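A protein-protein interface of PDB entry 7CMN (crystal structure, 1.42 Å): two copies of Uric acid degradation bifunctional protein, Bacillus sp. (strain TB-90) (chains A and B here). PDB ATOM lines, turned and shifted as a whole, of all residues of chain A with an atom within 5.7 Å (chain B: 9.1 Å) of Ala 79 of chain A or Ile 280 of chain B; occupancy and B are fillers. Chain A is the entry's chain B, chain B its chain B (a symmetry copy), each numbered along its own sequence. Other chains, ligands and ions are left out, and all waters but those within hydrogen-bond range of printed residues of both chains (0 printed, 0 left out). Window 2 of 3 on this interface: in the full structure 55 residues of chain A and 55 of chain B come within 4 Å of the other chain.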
ATOM      1  N   ARG A  14      25.654  11.098  14.909  1.00  0.00           N
ATOM      2  CA  ARG A  14      24.786  11.332  13.761  1.00  0.00           C
ATOM      3  C   ARG A  14      23.972  10.067  13.505  1.00  0.00           C
ATOM      4  O   ARG A  14      24.516   8.941  13.545  1.00  0.00           O
ATOM      5  CB  ARG A  14      25.680  11.617  12.543  1.00  0.00           C
ATOM      6  CG  ARG A  14      25.044  11.446  11.180  1.00  0.00           C
ATOM      7  CD  ARG A  14      24.233  12.655  10.738  1.00  0.00           C
ATOM      8  NE  ARG A  14      23.575  12.399   9.459  1.00  0.00           N
ATOM      9  CZ  ARG A  14      24.009  12.797   8.263  1.00  0.00           C
ATOM     10  NH1 ARG A  14      25.124  13.507   8.111  1.00  0.00           N
ATOM     11  NH2 ARG A  14      23.293  12.480   7.185  1.00  0.00           N
ATOM     12  N   THR A  15      22.690  10.243  13.231  1.00  0.00           N
ATOM     13  CA  THR A  15      21.864   9.131  12.789  1.00  0.00           C
ATOM     14  C   THR A  15      21.707   9.165  11.282  1.00  0.00           C
ATOM     15  O   THR A  15      21.631  10.248  10.665  1.00  0.00           O
ATOM     16  CB  THR A  15      20.508   9.111  13.483  1.00  0.00           C
ATOM     17  OG1 THR A  15      19.868  10.388  13.397  1.00  0.00           O
ATOM     18  CG2 THR A  15      20.615   8.751  14.924  1.00  0.00           C
ATOM     19  N   ILE A  74      32.593  21.525  14.185  1.00  0.00           N
ATOM     20  CA  ILE A  74      32.655  20.081  13.990  1.00  0.00           C
ATOM     21  C   ILE A  74      31.260  19.465  13.974  1.00  0.00           C
ATOM     22  O   ILE A  74      30.926  18.661  13.088  1.00  0.00           O
ATOM     23  CB  ILE A  74      33.566  19.453  15.054  1.00  0.00           C
ATOM     24  CG1 ILE A  74      35.005  19.907  14.838  1.00  0.00           C
ATOM     25  CG2 ILE A  74      33.466  17.923  15.014  1.00  0.00           C
ATOM     26  CD1 ILE A  74      35.881  19.703  16.028  1.00  0.00           C
ATOM     27  N   GLN A  75      30.433  19.817  14.959  1.00  0.00           N
ATOM     28  CA  GLN A  75      29.131  19.177  15.105  1.00  0.00           C
ATOM     29  C   GLN A  75      28.176  19.566  13.969  1.00  0.00           C
ATOM     30  O   GLN A  75      27.471  18.694  13.430  1.00  0.00           O
ATOM     31  CB  GLN A  75      28.543  19.555  16.482  1.00  0.00           C
ATOM     32  CG  GLN A  75      29.420  19.029  17.612  1.00  0.00           C
ATOM     33  CD  GLN A  75      28.934  19.431  18.993  1.00  0.00           C
ATOM     34  OE1 GLN A  75      28.203  20.394  19.145  1.00  0.00           O
ATOM     35  NE2 GLN A  75      29.366  18.682  20.003  1.00  0.00           N
ATOM     36  N   LYS A  76      28.237  20.810  13.508  1.00  0.00           N
ATOM     37  CA  LYS A  76      27.418  21.230  12.383  1.00  0.00           C
ATOM     38  C   LYS A  76      27.858  20.530  11.098  1.00  0.00           C
ATOM     39  O   LYS A  76      27.018  20.152  10.264  1.00  0.00           O
ATOM     40  CB  LYS A  76      27.512  22.741  12.197  1.00  0.00           C
ATOM     41  CG  LYS A  76      26.653  23.540  13.192  1.00  0.00           C
ATOM     42  CD  LYS A  76      25.162  23.322  12.952  1.00  0.00           C
ATOM     43  CE  LYS A  76      24.690  23.983  11.652  1.00  0.00           C
ATOM     44  NZ  LYS A  76      23.504  23.286  11.067  1.00  0.00           N
ATOM     45  N   HIS A  77      29.163  20.362  10.908  1.00  0.00           N
ATOM     46  CA  HIS A  77      29.624  19.692   9.695  1.00  0.00           C
ATOM     47  C   HIS A  77      29.296  18.205   9.688  1.00  0.00           C
ATOM     48  O   HIS A  77      29.123  17.642   8.618  1.00  0.00           O
ATOM     49  CB  HIS A  77      31.107  19.924   9.479  1.00  0.00           C
ATOM     50  CG  HIS A  77      31.395  21.257   8.869  1.00  0.00           C
ATOM     51  ND1 HIS A  77      31.317  22.440   9.582  1.00  0.00           N
ATOM     52  CD2 HIS A  77      31.732  21.603   7.606  1.00  0.00           C
ATOM     53  CE1 HIS A  77      31.599  23.453   8.777  1.00  0.00           C
ATOM     54  NE2 HIS A  77      31.869  22.969   7.579  1.00  0.00           N
ATOM     55  N   LEU A  78      29.158  17.569  10.849  1.00  0.00           N
ATOM     56  CA  LEU A  78      28.726  16.169  10.825  1.00  0.00           C
ATOM     57  C   LEU A  78      27.296  16.077  10.303  1.00  0.00           C
ATOM     58  O   LEU A  78      26.923  15.062   9.662  1.00  0.00           O
ATOM     59  CB  LEU A  78      28.828  15.532  12.219  1.00  0.00           C
ATOM     60  CG  LEU A  78      28.504  14.025  12.238  1.00  0.00           C
ATOM     61  CD1 LEU A  78      29.379  13.271  11.269  1.00  0.00           C
ATOM     62  CD2 LEU A  78      28.658  13.519  13.642  1.00  0.00           C
ATOM     63  N   ALA A  79      26.493  17.107  10.552  1.00  0.00           N
ATOM     64  CA  ALA A  79      25.124  17.149  10.031  1.00  0.00           C
ATOM     65  C   ALA A  79      25.124  17.246   8.505  1.00  0.00           C
ATOM     66  O   ALA A  79      24.299  16.626   7.841  1.00  0.00           O
ATOM     67  CB  ALA A  79      24.333  18.274  10.690  1.00  0.00           C
ATOM     68  N   SER A  80      26.020  18.058   7.932  1.00  0.00           N
ATOM     69  CA  SER A  80      26.054  18.289   6.504  1.00  0.00           C
ATOM     70  C   SER A  80      26.947  17.319   5.747  1.00  0.00           C
ATOM     71  O   SER A  80      26.973  17.374   4.519  1.00  0.00           O
ATOM     72  CB  SER A  80      26.476  19.744   6.194  1.00  0.00           C
ATOM     73  OG  SER A  80      27.745  20.030   6.762  1.00  0.00           O
ATOM     74  N   TYR A  81      27.660  16.441   6.446  1.00  0.00           N
ATOM     75  CA  TYR A  81      28.551  15.496   5.761  1.00  0.00           C
ATOM     76  C   TYR A  81      27.739  14.456   4.981  1.00  0.00           C
ATOM     77  O   TYR A  81      26.786  13.871   5.507  1.00  0.00           O
ATOM     78  CB  TYR A  81      29.454  14.798   6.789  1.00  0.00           C
ATOM     79  CG  TYR A  81      30.420  13.765   6.204  1.00  0.00           C
ATOM     80  CD1 TYR A  81      31.293  14.110   5.178  1.00  0.00           C
ATOM     81  CD2 TYR A  81      30.482  12.484   6.702  1.00  0.00           C
ATOM     82  CE1 TYR A  81      32.163  13.192   4.627  1.00  0.00           C
ATOM     83  CE2 TYR A  81      31.398  11.521   6.151  1.00  0.00           C
ATOM     84  CZ  TYR A  81      32.215  11.907   5.146  1.00  0.00           C
ATOM     85  OH  TYR A  81      33.063  10.965   4.597  1.00  0.00           O
ATOM     86  N   ILE B 276      21.658  18.692  18.851  1.00  0.00           N
ATOM     87  CA  ILE B 276      22.348  19.845  18.294  1.00  0.00           C
ATOM     88  C   ILE B 276      21.741  20.263  16.964  1.00  0.00           C
ATOM     89  O   ILE B 276      21.593  21.452  16.696  1.00  0.00           O
ATOM     90  CB  ILE B 276      23.859  19.530  18.132  1.00  0.00           C
ATOM     91  CG1 ILE B 276      24.463  19.154  19.478  1.00  0.00           C
ATOM     92  CG2 ILE B 276      24.580  20.720  17.526  1.00  0.00           C
ATOM     93  CD1 ILE B 276      24.306  20.179  20.555  1.00  0.00           C
ATOM     94  N   VAL B 277      21.427  19.298  16.100  1.00  0.00           N
ATOM     95  CA  VAL B 277      20.792  19.557  14.810  1.00  0.00           C
ATOM     96  C   VAL B 277      19.532  18.709  14.738  1.00  0.00           C
ATOM     97  O   VAL B 277      19.608  17.472  14.765  1.00  0.00           O
ATOM     98  CB  VAL B 277      21.727  19.231  13.624  1.00  0.00           C
ATOM     99  CG1 VAL B 277      21.036  19.533  12.297  1.00  0.00           C
ATOM    100  CG2 VAL B 277      23.024  20.009  13.753  1.00  0.00           C
ATOM    101  N   GLU B 278      18.378  19.377  14.654  1.00  0.00           N
ATOM    102  CA  GLU B 278      17.074  18.716  14.630  1.00  0.00           C
ATOM    103  C   GLU B 278      16.660  18.308  13.226  1.00  0.00           C
ATOM    104  O   GLU B 278      15.906  17.342  13.071  1.00  0.00           O
ATOM    105  CB  GLU B 278      16.013  19.661  15.222  1.00  0.00           C
ATOM    106  CG  GLU B 278      14.557  19.371  14.839  1.00  0.00           C
ATOM    107  CD  GLU B 278      13.986  18.129  15.513  1.00  0.00           C
ATOM    108  OE1 GLU B 278      14.624  17.611  16.453  1.00  0.00           O
ATOM    109  OE2 GLU B 278      12.897  17.668  15.094  1.00  0.00           O
ATOM    110  N   GLU B 279      17.125  19.021  12.204  1.00  0.00           N
ATOM    111  CA  GLU B 279      16.716  18.775  10.831  1.00  0.00           C
ATOM    112  C   GLU B 279      17.959  18.717   9.956  1.00  0.00           C
ATOM    113  O   GLU B 279      18.857  19.556  10.087  1.00  0.00           O
ATOM    114  CB  GLU B 279      15.778  19.888  10.326  1.00  0.00           C
ATOM    115  N   ILE B 280      18.013  17.724   9.079  1.00  0.00           N
ATOM    116  CA  ILE B 280      19.089  17.569   8.109  1.00  0.00           C
ATOM    117  C   ILE B 280      18.453  17.496   6.724  1.00  0.00           C
ATOM    118  O   ILE B 280      17.588  16.646   6.488  1.00  0.00           O
ATOM    119  CB  ILE B 280      19.940  16.321   8.390  1.00  0.00           C
ATOM    120  CG1 ILE B 280      20.629  16.454   9.747  1.00  0.00           C
ATOM    121  CG2 ILE B 280      20.969  16.115   7.284  1.00  0.00           C
ATOM    122  CD1 ILE B 280      21.502  15.250  10.118  1.00  0.00           C
ATOM    123  N   PRO B 281      18.828  18.363   5.787  1.00  0.00           N
ATOM    124  CA  PRO B 281      18.240  18.298   4.446  1.00  0.00           C
ATOM    125  C   PRO B 281      18.302  16.899   3.850  1.00  0.00           C
ATOM    126  O   PRO B 281      19.357  16.263   3.810  1.00  0.00           O
ATOM    127  CB  PRO B 281      19.092  19.283   3.636  1.00  0.00           C
ATOM    128  CG  PRO B 281      19.623  20.258   4.633  1.00  0.00           C
ATOM    129  CD  PRO B 281      19.664  19.568   5.979  1.00  0.00           C
ATOM    130  N   GLU B 282      17.149  16.417   3.388  1.00  0.00           N
ATOM    131  CA  GLU B 282      17.067  15.171   2.630  1.00  0.00           C
ATOM    132  C   GLU B 282      17.487  13.969   3.468  1.00  0.00           C
ATOM    133  O   GLU B 282      18.125  13.039   2.971  1.00  0.00           O
ATOM    134  CB  GLU B 282      17.886  15.246   1.336  1.00  0.00           C
ATOM    135  N   SER B 283      17.128  13.984   4.750  1.00  0.00           N
ATOM    136  CA  SER B 283      17.471  12.883   5.635  1.00  0.00           C
ATOM    137  C   SER B 283      16.603  12.945   6.881  1.00  0.00           C
ATOM    138  O   SER B 283      16.205  14.026   7.324  1.00  0.00           O
ATOM    139  CB  SER B 283      18.955  12.923   6.038  1.00  0.00           C
ATOM    140  OG  SER B 283      19.240  11.938   7.027  1.00  0.00           O
ATOM    141  N   GLU B 284      16.325  11.767   7.443  1.00  0.00           N
ATOM    142  CA  GLU B 284      15.703  11.662   8.757  1.00  0.00           C
ATOM    143  C   GLU B 284      16.719  11.752   9.895  1.00  0.00           C
ATOM    144  O   GLU B 284      16.332  11.634  11.064  1.00  0.00           O
ATOM    145  CB  GLU B 284      14.941  10.339   8.866  1.00  0.00           C
ATOM    146  N   GLY B 285      17.998  11.976   9.584  1.00  0.00           N
ATOM    147  CA  GLY B 285      19.030  11.984  10.597  1.00  0.00           C
ATOM    148  C   GLY B 285      19.090  13.294  11.379  1.00  0.00           C
ATOM    149  O   GLY B 285      18.504  14.333  11.014  1.00  0.00           O
ATOM    150  N   LYS B 286      19.813  13.228  12.485  1.00  0.00           N
ATOM    151  CA  LYS B 286      19.999  14.346  13.406  1.00  0.00           C
ATOM    152  C   LYS B 286      21.412  14.234  13.958  1.00  0.00           C
ATOM    153  O   LYS B 286      22.073  13.202  13.775  1.00  0.00           O
ATOM    154  CB  LYS B 286      18.984  14.267  14.539  1.00  0.00           C
ATOM    155  CG  LYS B 286      17.549  14.550  14.095  1.00  0.00           C
ATOM    156  CD  LYS B 286      16.561  14.215  15.208  1.00  0.00           C
ATOM    157  CE  LYS B 286      15.126  14.213  14.700  1.00  0.00           C
ATOM    158  NZ  LYS B 286      14.151  14.140  15.831  1.00  0.00           N
ATOM    159  N   VAL B 287      21.859  15.284  14.660  1.00  0.00           N
ATOM    160  CA  VAL B 287      23.147  15.248  15.356  1.00  0.00           C
ATOM    161  C   VAL B 287      22.964  15.557  16.838  1.00  0.00           C
ATOM    162  O   VAL B 287      22.269  16.507  17.222  1.00  0.00           O
ATOM    163  CB  VAL B 287      24.201  16.182  14.720  1.00  0.00           C
ATOM    164  CG1 VAL B 287      25.511  16.129  15.519  1.00  0.00           C
ATOM    165  CG2 VAL B 287      24.451  15.756  13.291  1.00  0.00           C
ATOM    166  N   TYR B 288      23.639  14.776  17.673  1.00  0.00           N
ATOM    167  CA  TYR B 288      23.576  14.886  19.111  1.00  0.00           C
ATOM    168  C   TYR B 288      24.983  14.928  19.678  1.00  0.00           C
ATOM    169  O   TYR B 288      25.960  14.654  18.992  1.00  0.00           O
ATOM    170  CB  TYR B 288      22.865  13.675  19.742  1.00  0.00           C
ATOM    171  CG  TYR B 288      21.519  13.359  19.153  1.00  0.00           C
ATOM    172  CD1 TYR B 288      20.358  13.821  19.744  1.00  0.00           C
ATOM    173  CD2 TYR B 288      21.404  12.536  18.046  1.00  0.00           C
ATOM    174  CE1 TYR B 288      19.117  13.529  19.215  1.00  0.00           C
ATOM    175  CE2 TYR B 288      20.179  12.227  17.506  1.00  0.00           C
ATOM    176  CZ  TYR B 288      19.032  12.714  18.097  1.00  0.00           C
ATOM    177  OH  TYR B 288      17.804  12.395  17.556  1.00  0.00           O
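Of the 13 printed residues of chain B, 6 touch a printed residue of chain A. Hydrophobic or aromatic side chains of chain A within 4 Å of the printed part of chain B: Ala 79.
O of Ala 79 of chain A is in hydrogen-bond range of NH1 of Arg 14 of chain A. The backbone carbonyl oxygen of Tyr 81 of chain A lies within hydrogen-bond range of the guanidinium group of Arg 14 of chain A, at 3.1 Å. The backbone carbonyl oxygen (O) of Val 287 of chain B lies within hydrogen-bond range of the backbone NH (N) of Ile 276 of chain B, at 2.8 Å. N of Val 277 of chain B lies within hydrogen-bond range of O of Val 287 of chain B, 3.1 Å away. The side-chain carboxylate (OE1) of Glu 278 of chain B is in salt-bridge range of the side-chain amino group (NZ) of Lys 286 of chain B (3.6 Å). OG of Ser 283 of chain B sits at hydrogen-bond distance from N of Gly 285 of chain B, at 2.8 Å.
No position is printed for both chains. Of the 9 pairs that touch across the chains among the printed residues, none has its exchanged pair printed and touching as well.
Arg 14 of chain A touches Ile 280 of chain B. CA of Arg 14 of chain A touches O of Lys 286 of chain B, 3.3 Å away. Thr 15 of chain A touches Gly 285 of chain B. OE1 of Gln 75 of chain A touches CG1 of Ile 276 of chain B (3.95 Å). CG1 of Val 287 of chain B touches O of Gln 75 of chain A, at 3.8 Å. Ala 79 of chain A touches Val 277 of chain B. O of Ala 79 of chain A touches CG2 of Ile 280 of chain B, at 3.4 Å. Ala 79 of chain A touches Val 287 of chain B (CA to CG2, 3.6 Å).
The backbone NH (N) of Lys 286 of chain B lies within hydrogen-bond range of the side-chain hydroxyl (OG1) of Thr 15 of chain A, 3.0 Å away.
Of the printed residues of chain B, Arg 14 of chain A touches Ile 280 (3.6 Å) and Lys 286 (3.3 Å). No residue of chain B comes within 4 Å of Ser 80 of chain A. Glu 279 of chain B touches none of the printed residues of chain A. Of the printed residues of chain A, Ile 280 of chain B touches Arg 14 and Ala 79. Glu 282 of chain B touches none of the printed residues of chain A. Printed residues of chain A within 4 Å of Lys 286 of chain B: Arg 14 and Thr 15. The nearest residue of chain A that does not touch Ile 280 of chain B is Thr 15 of chain A (5.0 Å).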
